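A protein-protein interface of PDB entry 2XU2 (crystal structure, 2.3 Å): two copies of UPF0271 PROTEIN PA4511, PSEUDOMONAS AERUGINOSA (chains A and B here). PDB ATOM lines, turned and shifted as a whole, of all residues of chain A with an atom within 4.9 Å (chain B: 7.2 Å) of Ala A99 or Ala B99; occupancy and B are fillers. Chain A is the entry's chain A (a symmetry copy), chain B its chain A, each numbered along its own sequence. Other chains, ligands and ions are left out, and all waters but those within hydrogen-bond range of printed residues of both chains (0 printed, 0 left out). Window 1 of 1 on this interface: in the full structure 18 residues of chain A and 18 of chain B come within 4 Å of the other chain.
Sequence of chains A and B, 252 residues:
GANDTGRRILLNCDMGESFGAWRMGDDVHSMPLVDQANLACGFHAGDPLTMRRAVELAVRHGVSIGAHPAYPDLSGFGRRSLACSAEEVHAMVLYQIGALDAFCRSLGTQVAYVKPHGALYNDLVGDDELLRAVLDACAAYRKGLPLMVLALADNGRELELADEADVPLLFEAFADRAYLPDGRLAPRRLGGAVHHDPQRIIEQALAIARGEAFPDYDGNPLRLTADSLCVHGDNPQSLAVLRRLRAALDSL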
ATOM      1  N   MET A  51      -5.664 -20.943   4.044  1.00  0.00           N
ATOM      2  CA  MET A  51      -5.890 -19.512   4.247  1.00  0.00           C
ATOM      3  C   MET A  51      -4.697 -18.682   3.809  1.00  0.00           C
ATOM      4  O   MET A  51      -4.858 -17.705   3.074  1.00  0.00           O
ATOM      5  CB  MET A  51      -6.228 -19.229   5.701  1.00  0.00           C
ATOM      6  CG  MET A  51      -7.606 -19.712   6.069  1.00  0.00           C
ATOM      7  SD  MET A  51      -7.932 -19.488   7.813  1.00  0.00           S
ATOM      8  CE  MET A  51      -8.082 -17.717   8.059  1.00  0.00           C
ATOM      9  N   TYR A  95     -13.321 -13.943  16.167  1.00  0.00           N
ATOM     10  CA  TYR A  95     -12.272 -14.951  16.098  1.00  0.00           C
ATOM     11  C   TYR A  95     -11.782 -15.146  14.664  1.00  0.00           C
ATOM     12  O   TYR A  95     -10.576 -15.166  14.395  1.00  0.00           O
ATOM     13  CB  TYR A  95     -12.836 -16.270  16.643  1.00  0.00           C
ATOM     14  CG  TYR A  95     -11.900 -17.450  16.634  1.00  0.00           C
ATOM     15  CD1 TYR A  95     -11.316 -17.909  17.812  1.00  0.00           C
ATOM     16  CD2 TYR A  95     -11.617 -18.131  15.460  1.00  0.00           C
ATOM     17  CE1 TYR A  95     -10.469 -19.009  17.814  1.00  0.00           C
ATOM     18  CE2 TYR A  95     -10.745 -19.249  15.462  1.00  0.00           C
ATOM     19  CZ  TYR A  95     -10.181 -19.677  16.643  1.00  0.00           C
ATOM     20  OH  TYR A  95      -9.328 -20.776  16.662  1.00  0.00           O
ATOM     21  N   GLN A  96     -12.738 -15.298  13.751  1.00  0.00           N
ATOM     22  CA  GLN A  96     -12.445 -15.622  12.372  1.00  0.00           C
ATOM     23  C   GLN A  96     -11.832 -14.458  11.604  1.00  0.00           C
ATOM     24  O   GLN A  96     -10.915 -14.649  10.796  1.00  0.00           O
ATOM     25  CB  GLN A  96     -13.712 -16.119  11.679  1.00  0.00           C
ATOM     26  CG  GLN A  96     -14.085 -17.548  12.085  1.00  0.00           C
ATOM     27  CD  GLN A  96     -15.422 -17.982  11.500  1.00  0.00           C
ATOM     28  OE1 GLN A  96     -15.492 -18.420  10.339  1.00  0.00           O
ATOM     29  NE2 GLN A  96     -16.491 -17.859  12.299  1.00  0.00           N
ATOM     30  N   ILE A  97     -12.329 -13.252  11.861  1.00  0.00           N
ATOM     31  CA  ILE A  97     -11.726 -12.052  11.280  1.00  0.00           C
ATOM     32  C   ILE A  97     -10.255 -11.919  11.695  1.00  0.00           C
ATOM     33  O   ILE A  97      -9.408 -11.639  10.861  1.00  0.00           O
ATOM     34  CB  ILE A  97     -12.462 -10.776  11.694  1.00  0.00           C
ATOM     35  CG1 ILE A  97     -13.874 -10.755  11.099  1.00  0.00           C
ATOM     36  CG2 ILE A  97     -11.654  -9.532  11.252  1.00  0.00           C
ATOM     37  CD1 ILE A  97     -14.726  -9.562  11.571  1.00  0.00           C
ATOM     38  N   GLY A  98      -9.966 -12.109  12.981  1.00  0.00           N
ATOM     39  CA  GLY A  98      -8.595 -11.990  13.481  1.00  0.00           C
ATOM     40  C   GLY A  98      -7.654 -13.068  12.952  1.00  0.00           C
ATOM     41  O   GLY A  98      -6.482 -12.798  12.689  1.00  0.00           O
ATOM     42  N   ALA A  99      -8.167 -14.289  12.793  1.00  0.00           N
ATOM     43  CA  ALA A  99      -7.372 -15.397  12.232  1.00  0.00           C
ATOM     44  C   ALA A  99      -6.928 -15.113  10.788  1.00  0.00           C
ATOM     45  O   ALA A  99      -5.749 -15.254  10.459  1.00  0.00           O
ATOM     46  CB  ALA A  99      -8.159 -16.690  12.304  1.00  0.00           C
ATOM     47  N   LEU A 100      -7.877 -14.704   9.941  1.00  0.00           N
ATOM     48  CA  LEU A 100      -7.581 -14.301   8.558  1.00  0.00           C
ATOM     49  C   LEU A 100      -6.694 -13.066   8.487  1.00  0.00           C
ATOM     50  O   LEU A 100      -5.729 -13.031   7.703  1.00  0.00           O
ATOM     51  CB  LEU A 100      -8.874 -14.041   7.763  1.00  0.00           C
ATOM     52  CG  LEU A 100      -8.664 -13.700   6.272  1.00  0.00           C
ATOM     53  CD1 LEU A 100      -8.014 -14.867   5.528  1.00  0.00           C
ATOM     54  CD2 LEU A 100      -9.974 -13.274   5.582  1.00  0.00           C
ATOM     55  N   ASP A 101      -7.000 -12.060   9.308  1.00  0.00           N
ATOM     56  CA  ASP A 101      -6.228 -10.817   9.301  1.00  0.00           C
ATOM     57  C   ASP A 101      -4.753 -11.042   9.673  1.00  0.00           C
ATOM     58  O   ASP A 101      -3.890 -10.255   9.274  1.00  0.00           O
ATOM     59  CB  ASP A 101      -6.843  -9.780  10.239  1.00  0.00           C
ATOM     60  CG  ASP A 101      -6.489  -8.330   9.853  1.00  0.00           C
ATOM     61  OD1 ASP A 101      -6.483  -7.995   8.650  1.00  0.00           O
ATOM     62  OD2 ASP A 101      -6.260  -7.507  10.766  1.00  0.00           O
ATOM     63  N   ALA A 102      -4.469 -12.103  10.432  1.00  0.00           N
ATOM     64  CA  ALA A 102      -3.088 -12.429  10.786  1.00  0.00           C
ATOM     65  C   ALA A 102      -2.292 -12.721   9.523  1.00  0.00           C
ATOM     66  O   ALA A 102      -1.145 -12.285   9.399  1.00  0.00           O
ATOM     67  CB  ALA A 102      -3.036 -13.610  11.735  1.00  0.00           C
ATOM     68  N   PHE A 103      -2.911 -13.441   8.582  1.00  0.00           N
ATOM     69  CA  PHE A 103      -2.253 -13.762   7.322  1.00  0.00           C
ATOM     70  C   PHE A 103      -2.157 -12.536   6.424  1.00  0.00           C
ATOM     71  O   PHE A 103      -1.124 -12.320   5.792  1.00  0.00           O
ATOM     72  CB  PHE A 103      -2.960 -14.903   6.611  1.00  0.00           C
ATOM     73  CG  PHE A 103      -2.887 -16.188   7.351  1.00  0.00           C
ATOM     74  CD1 PHE A 103      -1.730 -16.955   7.317  1.00  0.00           C
ATOM     75  CD2 PHE A 103      -3.963 -16.633   8.103  1.00  0.00           C
ATOM     76  CE1 PHE A 103      -1.653 -18.158   8.016  1.00  0.00           C
ATOM     77  CE2 PHE A 103      -3.889 -17.834   8.810  1.00  0.00           C
ATOM     78  CZ  PHE A 103      -2.746 -18.591   8.758  1.00  0.00           C
ATOM     79  N   CYS B  41      -6.421 -21.224  22.146  1.00  0.00           N
ATOM     80  CA  CYS B  41      -6.826 -20.541  20.910  1.00  0.00           C
ATOM     81  C   CYS B  41      -7.743 -21.385  20.005  1.00  0.00           C
ATOM     82  O   CYS B  41      -7.829 -21.125  18.807  1.00  0.00           O
ATOM     83  CB  CYS B  41      -5.584 -20.079  20.149  1.00  0.00           C
ATOM     84  SG  CYS B  41      -4.457 -18.983  21.103  1.00  0.00           S
ATOM     85  N   GLY B  42      -8.415 -22.393  20.575  1.00  0.00           N
ATOM     86  CA  GLY B  42      -9.433 -23.152  19.863  1.00  0.00           C
ATOM     87  C   GLY B  42      -8.990 -24.430  19.182  1.00  0.00           C
ATOM     88  O   GLY B  42      -9.813 -25.117  18.579  1.00  0.00           O
ATOM     89  N   PHE B  43      -7.704 -24.760  19.276  1.00  0.00           N
ATOM     90  CA  PHE B  43      -7.168 -25.944  18.611  1.00  0.00           C
ATOM     91  C   PHE B  43      -7.100 -27.124  19.570  1.00  0.00           C
ATOM     92  O   PHE B  43      -7.303 -28.262  19.150  1.00  0.00           O
ATOM     93  CB  PHE B  43      -5.788 -25.655  17.998  1.00  0.00           C
ATOM     94  CG  PHE B  43      -5.853 -25.012  16.649  1.00  0.00           C
ATOM     95  CD1 PHE B  43      -6.525 -23.802  16.471  1.00  0.00           C
ATOM     96  CD2 PHE B  43      -5.275 -25.620  15.542  1.00  0.00           C
ATOM     97  CE1 PHE B  43      -6.602 -23.209  15.233  1.00  0.00           C
ATOM     98  CE2 PHE B  43      -5.361 -25.028  14.278  1.00  0.00           C
ATOM     99  CZ  PHE B  43      -6.016 -23.811  14.131  1.00  0.00           C
ATOM    100  N   MET B  51     -12.779 -17.963  25.005  1.00  0.00           N
ATOM    101  CA  MET B  51     -11.638 -17.075  24.782  1.00  0.00           C
ATOM    102  C   MET B  51     -11.939 -15.648  25.202  1.00  0.00           C
ATOM    103  O   MET B  51     -11.151 -15.034  25.924  1.00  0.00           O
ATOM    104  CB  MET B  51     -11.206 -17.120  23.327  1.00  0.00           C
ATOM    105  CG  MET B  51     -10.531 -18.420  22.973  1.00  0.00           C
ATOM    106  SD  MET B  51     -10.150 -18.503  21.228  1.00  0.00           S
ATOM    107  CE  MET B  51      -8.832 -17.316  20.957  1.00  0.00           C
ATOM    108  N   ALA B  91       1.596 -21.660   9.987  1.00  0.00           N
ATOM    109  CA  ALA B  91       0.264 -21.137   9.702  1.00  0.00           C
ATOM    110  C   ALA B  91      -0.739 -21.316  10.853  1.00  0.00           C
ATOM    111  O   ALA B  91      -1.565 -20.440  11.104  1.00  0.00           O
ATOM    112  CB  ALA B  91      -0.294 -21.766   8.407  1.00  0.00           C
ATOM    113  N   VAL B  93       0.008 -21.491  14.032  1.00  0.00           N
ATOM    114  CA  VAL B  93       0.417 -20.580  15.108  1.00  0.00           C
ATOM    115  C   VAL B  93      -0.062 -19.169  14.798  1.00  0.00           C
ATOM    116  O   VAL B  93      -0.679 -18.521  15.643  1.00  0.00           O
ATOM    117  CB  VAL B  93       1.951 -20.605  15.343  1.00  0.00           C
ATOM    118  CG1 VAL B  93       2.378 -19.496  16.314  1.00  0.00           C
ATOM    119  CG2 VAL B  93       2.355 -21.954  15.897  1.00  0.00           C
ATOM    120  N   LEU B  94       0.197 -18.713  13.573  1.00  0.00           N
ATOM    121  CA  LEU B  94      -0.221 -17.396  13.143  1.00  0.00           C
ATOM    122  C   LEU B  94      -1.739 -17.234  13.281  1.00  0.00           C
ATOM    123  O   LEU B  94      -2.229 -16.208  13.777  1.00  0.00           O
ATOM    124  CB  LEU B  94       0.223 -17.152  11.694  1.00  0.00           C
ATOM    125  CG  LEU B  94       0.279 -15.710  11.188  1.00  0.00           C
ATOM    126  CD1 LEU B  94       0.964 -14.773  12.210  1.00  0.00           C
ATOM    127  CD2 LEU B  94       0.999 -15.666   9.829  1.00  0.00           C
ATOM    128  N   TYR B  95      -2.473 -18.252  12.826  1.00  0.00           N
ATOM    129  CA  TYR B  95      -3.927 -18.271  12.904  1.00  0.00           C
ATOM    130  C   TYR B  95      -4.410 -18.059  14.338  1.00  0.00           C
ATOM    131  O   TYR B  95      -5.303 -17.246  14.600  1.00  0.00           O
ATOM    132  CB  TYR B  95      -4.420 -19.627  12.381  1.00  0.00           C
ATOM    133  CG  TYR B  95      -5.909 -19.849  12.401  1.00  0.00           C
ATOM    134  CD1 TYR B  95      -6.655 -19.802  11.227  1.00  0.00           C
ATOM    135  CD2 TYR B  95      -6.574 -20.137  13.583  1.00  0.00           C
ATOM    136  CE1 TYR B  95      -8.026 -20.028  11.236  1.00  0.00           C
ATOM    137  CE2 TYR B  95      -7.975 -20.358  13.592  1.00  0.00           C
ATOM    138  CZ  TYR B  95      -8.686 -20.302  12.414  1.00  0.00           C
ATOM    139  OH  TYR B  95     -10.060 -20.522  12.406  1.00  0.00           O
ATOM    140  N   GLN B  96      -3.811 -18.810  15.258  1.00  0.00           N
ATOM    141  CA  GLN B  96      -4.239 -18.827  16.640  1.00  0.00           C
ATOM    142  C   GLN B  96      -3.887 -17.547  17.388  1.00  0.00           C
ATOM    143  O   GLN B  96      -4.683 -17.049  18.193  1.00  0.00           O
ATOM    144  CB  GLN B  96      -3.649 -20.046  17.347  1.00  0.00           C
ATOM    145  CG  GLN B  96      -4.354 -21.349  16.963  1.00  0.00           C
ATOM    146  CD  GLN B  96      -3.671 -22.571  17.562  1.00  0.00           C
ATOM    147  OE1 GLN B  96      -3.913 -22.922  18.729  1.00  0.00           O
ATOM    148  NE2 GLN B  96      -2.811 -23.223  16.768  1.00  0.00           N
ATOM    149  N   ILE B  97      -2.701 -17.009  17.117  1.00  0.00           N
ATOM    150  CA  ILE B  97      -2.319 -15.713  17.677  1.00  0.00           C
ATOM    151  C   ILE B  97      -3.305 -14.617  17.252  1.00  0.00           C
ATOM    152  O   ILE B  97      -3.728 -13.823  18.078  1.00  0.00           O
ATOM    153  CB  ILE B  97      -0.912 -15.290  17.249  1.00  0.00           C
ATOM    154  CG1 ILE B  97       0.136 -16.230  17.852  1.00  0.00           C
ATOM    155  CG2 ILE B  97      -0.650 -13.823  17.669  1.00  0.00           C
ATOM    156  CD1 ILE B  97       1.571 -15.948  17.368  1.00  0.00           C
ATOM    157  N   GLY B  98      -3.653 -14.576  15.968  1.00  0.00           N
ATOM    158  CA  GLY B  98      -4.576 -13.560  15.458  1.00  0.00           C
ATOM    159  C   GLY B  98      -5.997 -13.697  15.997  1.00  0.00           C
ATOM    160  O   GLY B  98      -6.667 -12.696  16.250  1.00  0.00           O
ATOM    161  N   ALA B  99      -6.455 -14.937  16.176  1.00  0.00           N
ATOM    162  CA  ALA B  99      -7.789 -15.195  16.748  1.00  0.00           C
ATOM    163  C   ALA B  99      -7.911 -14.665  18.186  1.00  0.00           C
ATOM    164  O   ALA B  99      -8.867 -13.957  18.510  1.00  0.00           O
ATOM    165  CB  ALA B  99      -8.098 -16.678  16.699  1.00  0.00           C
ATOM    166  N   LEU B 100      -6.934 -15.002  19.032  1.00  0.00           N
ATOM    167  CA  LEU B 100      -6.868 -14.486  20.408  1.00  0.00           C
ATOM    168  C   LEU B 100      -6.671 -12.977  20.456  1.00  0.00           C
ATOM    169  O   LEU B 100      -7.348 -12.281  21.235  1.00  0.00           O
ATOM    170  CB  LEU B 100      -5.741 -15.168  21.206  1.00  0.00           C
ATOM    171  CG  LEU B 100      -5.654 -14.754  22.691  1.00  0.00           C
ATOM    172  CD1 LEU B 100      -6.921 -15.152  23.448  1.00  0.00           C
ATOM    173  CD2 LEU B 100      -4.402 -15.328  23.382  1.00  0.00           C
ATOM    174  N   ASP B 101      -5.765 -12.464  19.622  1.00  0.00           N
ATOM    175  CA  ASP B 101      -5.480 -11.028  19.608  1.00  0.00           C
ATOM    176  C   ASP B 101      -6.713 -10.191  19.231  1.00  0.00           C
ATOM    177  O   ASP B 101      -6.804  -9.020  19.614  1.00  0.00           O
ATOM    178  CB  ASP B 101      -4.329 -10.704  18.659  1.00  0.00           C
ATOM    179  CG  ASP B 101      -3.593  -9.398  19.023  1.00  0.00           C
ATOM    180  OD1 ASP B 101      -3.363  -9.132  20.220  1.00  0.00           O
ATOM    181  OD2 ASP B 101      -3.204  -8.653  18.096  1.00  0.00           O
ATOM    182  N   ALA B 102      -7.650 -10.782  18.485  1.00  0.00           N
ATOM    183  CA  ALA B 102      -8.882 -10.082  18.129  1.00  0.00           C
ATOM    184  C   ALA B 102      -9.657  -9.734  19.391  1.00  0.00           C
ATOM    185  O   ALA B 102     -10.196  -8.630  19.502  1.00  0.00           O
ATOM    186  CB  ALA B 102      -9.732 -10.922  17.196  1.00  0.00           C
ATOM    187  N   PHE B 103      -9.691 -10.668  20.345  1.00  0.00           N
ATOM    188  CA  PHE B 103     -10.384 -10.436  21.606  1.00  0.00           C
ATOM    189  C   PHE B 103      -9.612  -9.462  22.486  1.00  0.00           C
ATOM    190  O   PHE B 103     -10.215  -8.590  23.109  1.00  0.00           O
ATOM    191  CB  PHE B 103     -10.642 -11.742  22.337  1.00  0.00           C
ATOM    192  CG  PHE B 103     -11.578 -12.641  21.615  1.00  0.00           C
ATOM    193  CD1 PHE B 103     -12.947 -12.410  21.654  1.00  0.00           C
ATOM    194  CD2 PHE B 103     -11.100 -13.711  20.875  1.00  0.00           C
ATOM    195  CE1 PHE B 103     -13.828 -13.246  20.971  1.00  0.00           C
ATOM    196  CE2 PHE B 103     -11.979 -14.548  20.185  1.00  0.00           C
ATOM    197  CZ  PHE B 103     -13.329 -14.319  20.241  1.00  0.00           C
ATOM    198  N   CYS B 104      -8.287  -9.588  22.501  1.00  0.00           N
ATOM    199  CA  CYS B 104      -7.429  -8.696  23.288  1.00  0.00           C
ATOM    200  C   CYS B 104      -7.647  -7.238  22.912  1.00  0.00           C
ATOM    201  O   CYS B 104      -7.908  -6.407  23.783  1.00  0.00           O
ATOM    202  CB  CYS B 104      -5.950  -9.066  23.130  1.00  0.00           C
ATOM    203  SG  CYS B 104      -5.501 -10.663  23.852  1.00  0.00           S
ATOM    204  N   VAL B 111      -2.014  -9.479  22.801  1.00  0.00           N
ATOM    205  CA  VAL B 111      -1.173 -10.651  23.098  1.00  0.00           C
ATOM    206  C   VAL B 111       0.265 -10.207  23.401  1.00  0.00           C
ATOM    207  O   VAL B 111       0.894  -9.535  22.587  1.00  0.00           O
ATOM    208  CB  VAL B 111      -1.211 -11.635  21.933  1.00  0.00           C
ATOM    209  CG1 VAL B 111      -0.110 -12.684  22.055  1.00  0.00           C
ATOM    210  CG2 VAL B 111      -2.611 -12.277  21.876  1.00  0.00           C
ATOM    211  N   TYR B 141       3.851 -11.926  13.094  1.00  0.00           N
ATOM    212  CA  TYR B 141       2.695 -11.299  13.723  1.00  0.00           C
ATOM    213  C   TYR B 141       3.024  -9.914  14.291  1.00  0.00           C
ATOM    214  O   TYR B 141       2.367  -8.942  13.941  1.00  0.00           O
ATOM    215  CB  TYR B 141       2.046 -12.180  14.791  1.00  0.00           C
ATOM    216  CG  TYR B 141       0.676 -11.638  15.132  1.00  0.00           C
ATOM    217  CD1 TYR B 141      -0.413 -11.923  14.319  1.00  0.00           C
ATOM    218  CD2 TYR B 141       0.484 -10.792  16.223  1.00  0.00           C
ATOM    219  CE1 TYR B 141      -1.675 -11.402  14.589  1.00  0.00           C
ATOM    220  CE2 TYR B 141      -0.775 -10.273  16.512  1.00  0.00           C
ATOM    221  CZ  TYR B 141      -1.849 -10.585  15.686  1.00  0.00           C
ATOM    222  OH  TYR B 141      -3.095 -10.088  15.938  1.00  0.00           O
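The side-chain hydroxyl (OH) of Tyr A95 is in hydrogen-bond range of the backbone carbonyl oxygen (O) of Cys B41.
The backbone carbonyl oxygen of Gln B96 sits at hydrogen-bond distance from the side-chain sulfur of Cys B41 (3.5 Å). The side-chain carboxylate (OD2) of Asp B101 lies within hydrogen-bond range of the side-chain hydroxyl (OH) of Tyr B141, 2.6 Å away.
Among the printed residues, merely in contact across the chains: Phe A103 with Ala B91 (3.2 Å), Tyr A95 with Tyr B95 (3.4 Å), Ala A102 with Leu B94 (3.4 Å), Gly A98 with Gly B98 (3.4 Å), Tyr A95 with Met B51 (3.5 Å), Met A51 with Tyr B95 (3.5 Å), Tyr A95 with Ala B99 (3.5 Å), Ala A99 with Tyr B95 (3.5 Å), Ala A99 with Ala B99 (3.8 Å), Ala A102 with Tyr B141 (3.9 Å), Gly A98 with Ala B99 (3.9 Å), Ala A99 with Gly B98 (3.9 Å), Tyr A95 with Phe B43 (3.9 Å), Phe A103 with Leu B94 (3.9 Å) and Tyr A95 with Gly B42 (3.99 Å).
Of the printed residues of chain B, Tyr A95 touches Cys B41, Gly B42, Phe B43, Met B51, Tyr B95 and Ala B99. Ile A97 touches none of the printed residues of chain B. Gly A98 touches just these residues of chain B: Gly B98 and Ala B99. Ala A99 touches three residues of chain B. Of the printed residues of chain B, Ala A102 touches Leu B94 (3.4 Å) and Tyr B141 (3.9 Å). Of chain A, only Tyr A95 (3.5 Å), Gly A98 (3.9 Å) and Ala A99 (3.8 Å) come within 4 Å of Ala B99. The nearest residue of chain B that does not touch Ala A99 is Leu B94 (4.9 Å). The nearest printed residue of chain A that does not touch Ala B99 is Gln A96 (5.7 Å).
Of the 10 printed residues of chain A, 6 touch a printed residue of chain B. Along chain B the printed residues that touch a printed residue of chain A span positions 41 to 141. Among the printed residues, 16 pairs touch across the chains. Among the printed residues, no Asp or Glu carboxylate lies within 4 Å of a Lys or Arg side-chain nitrogen of the other chain.
Tyr A95 touches its own counterpart, Tyr B95. Tyr A95 touches Ala B99, and with the chains exchanged Ala A99 touches Tyr B95. Gly B98 touches its own counterpart, Gly A98. Ala A99 touches its own counterpart, Ala B99. 10 positions are printed for both chains. Of the 16 pairs that touch across the chains among the printed residues, 9 have their exchanged pair printed and touching as well.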
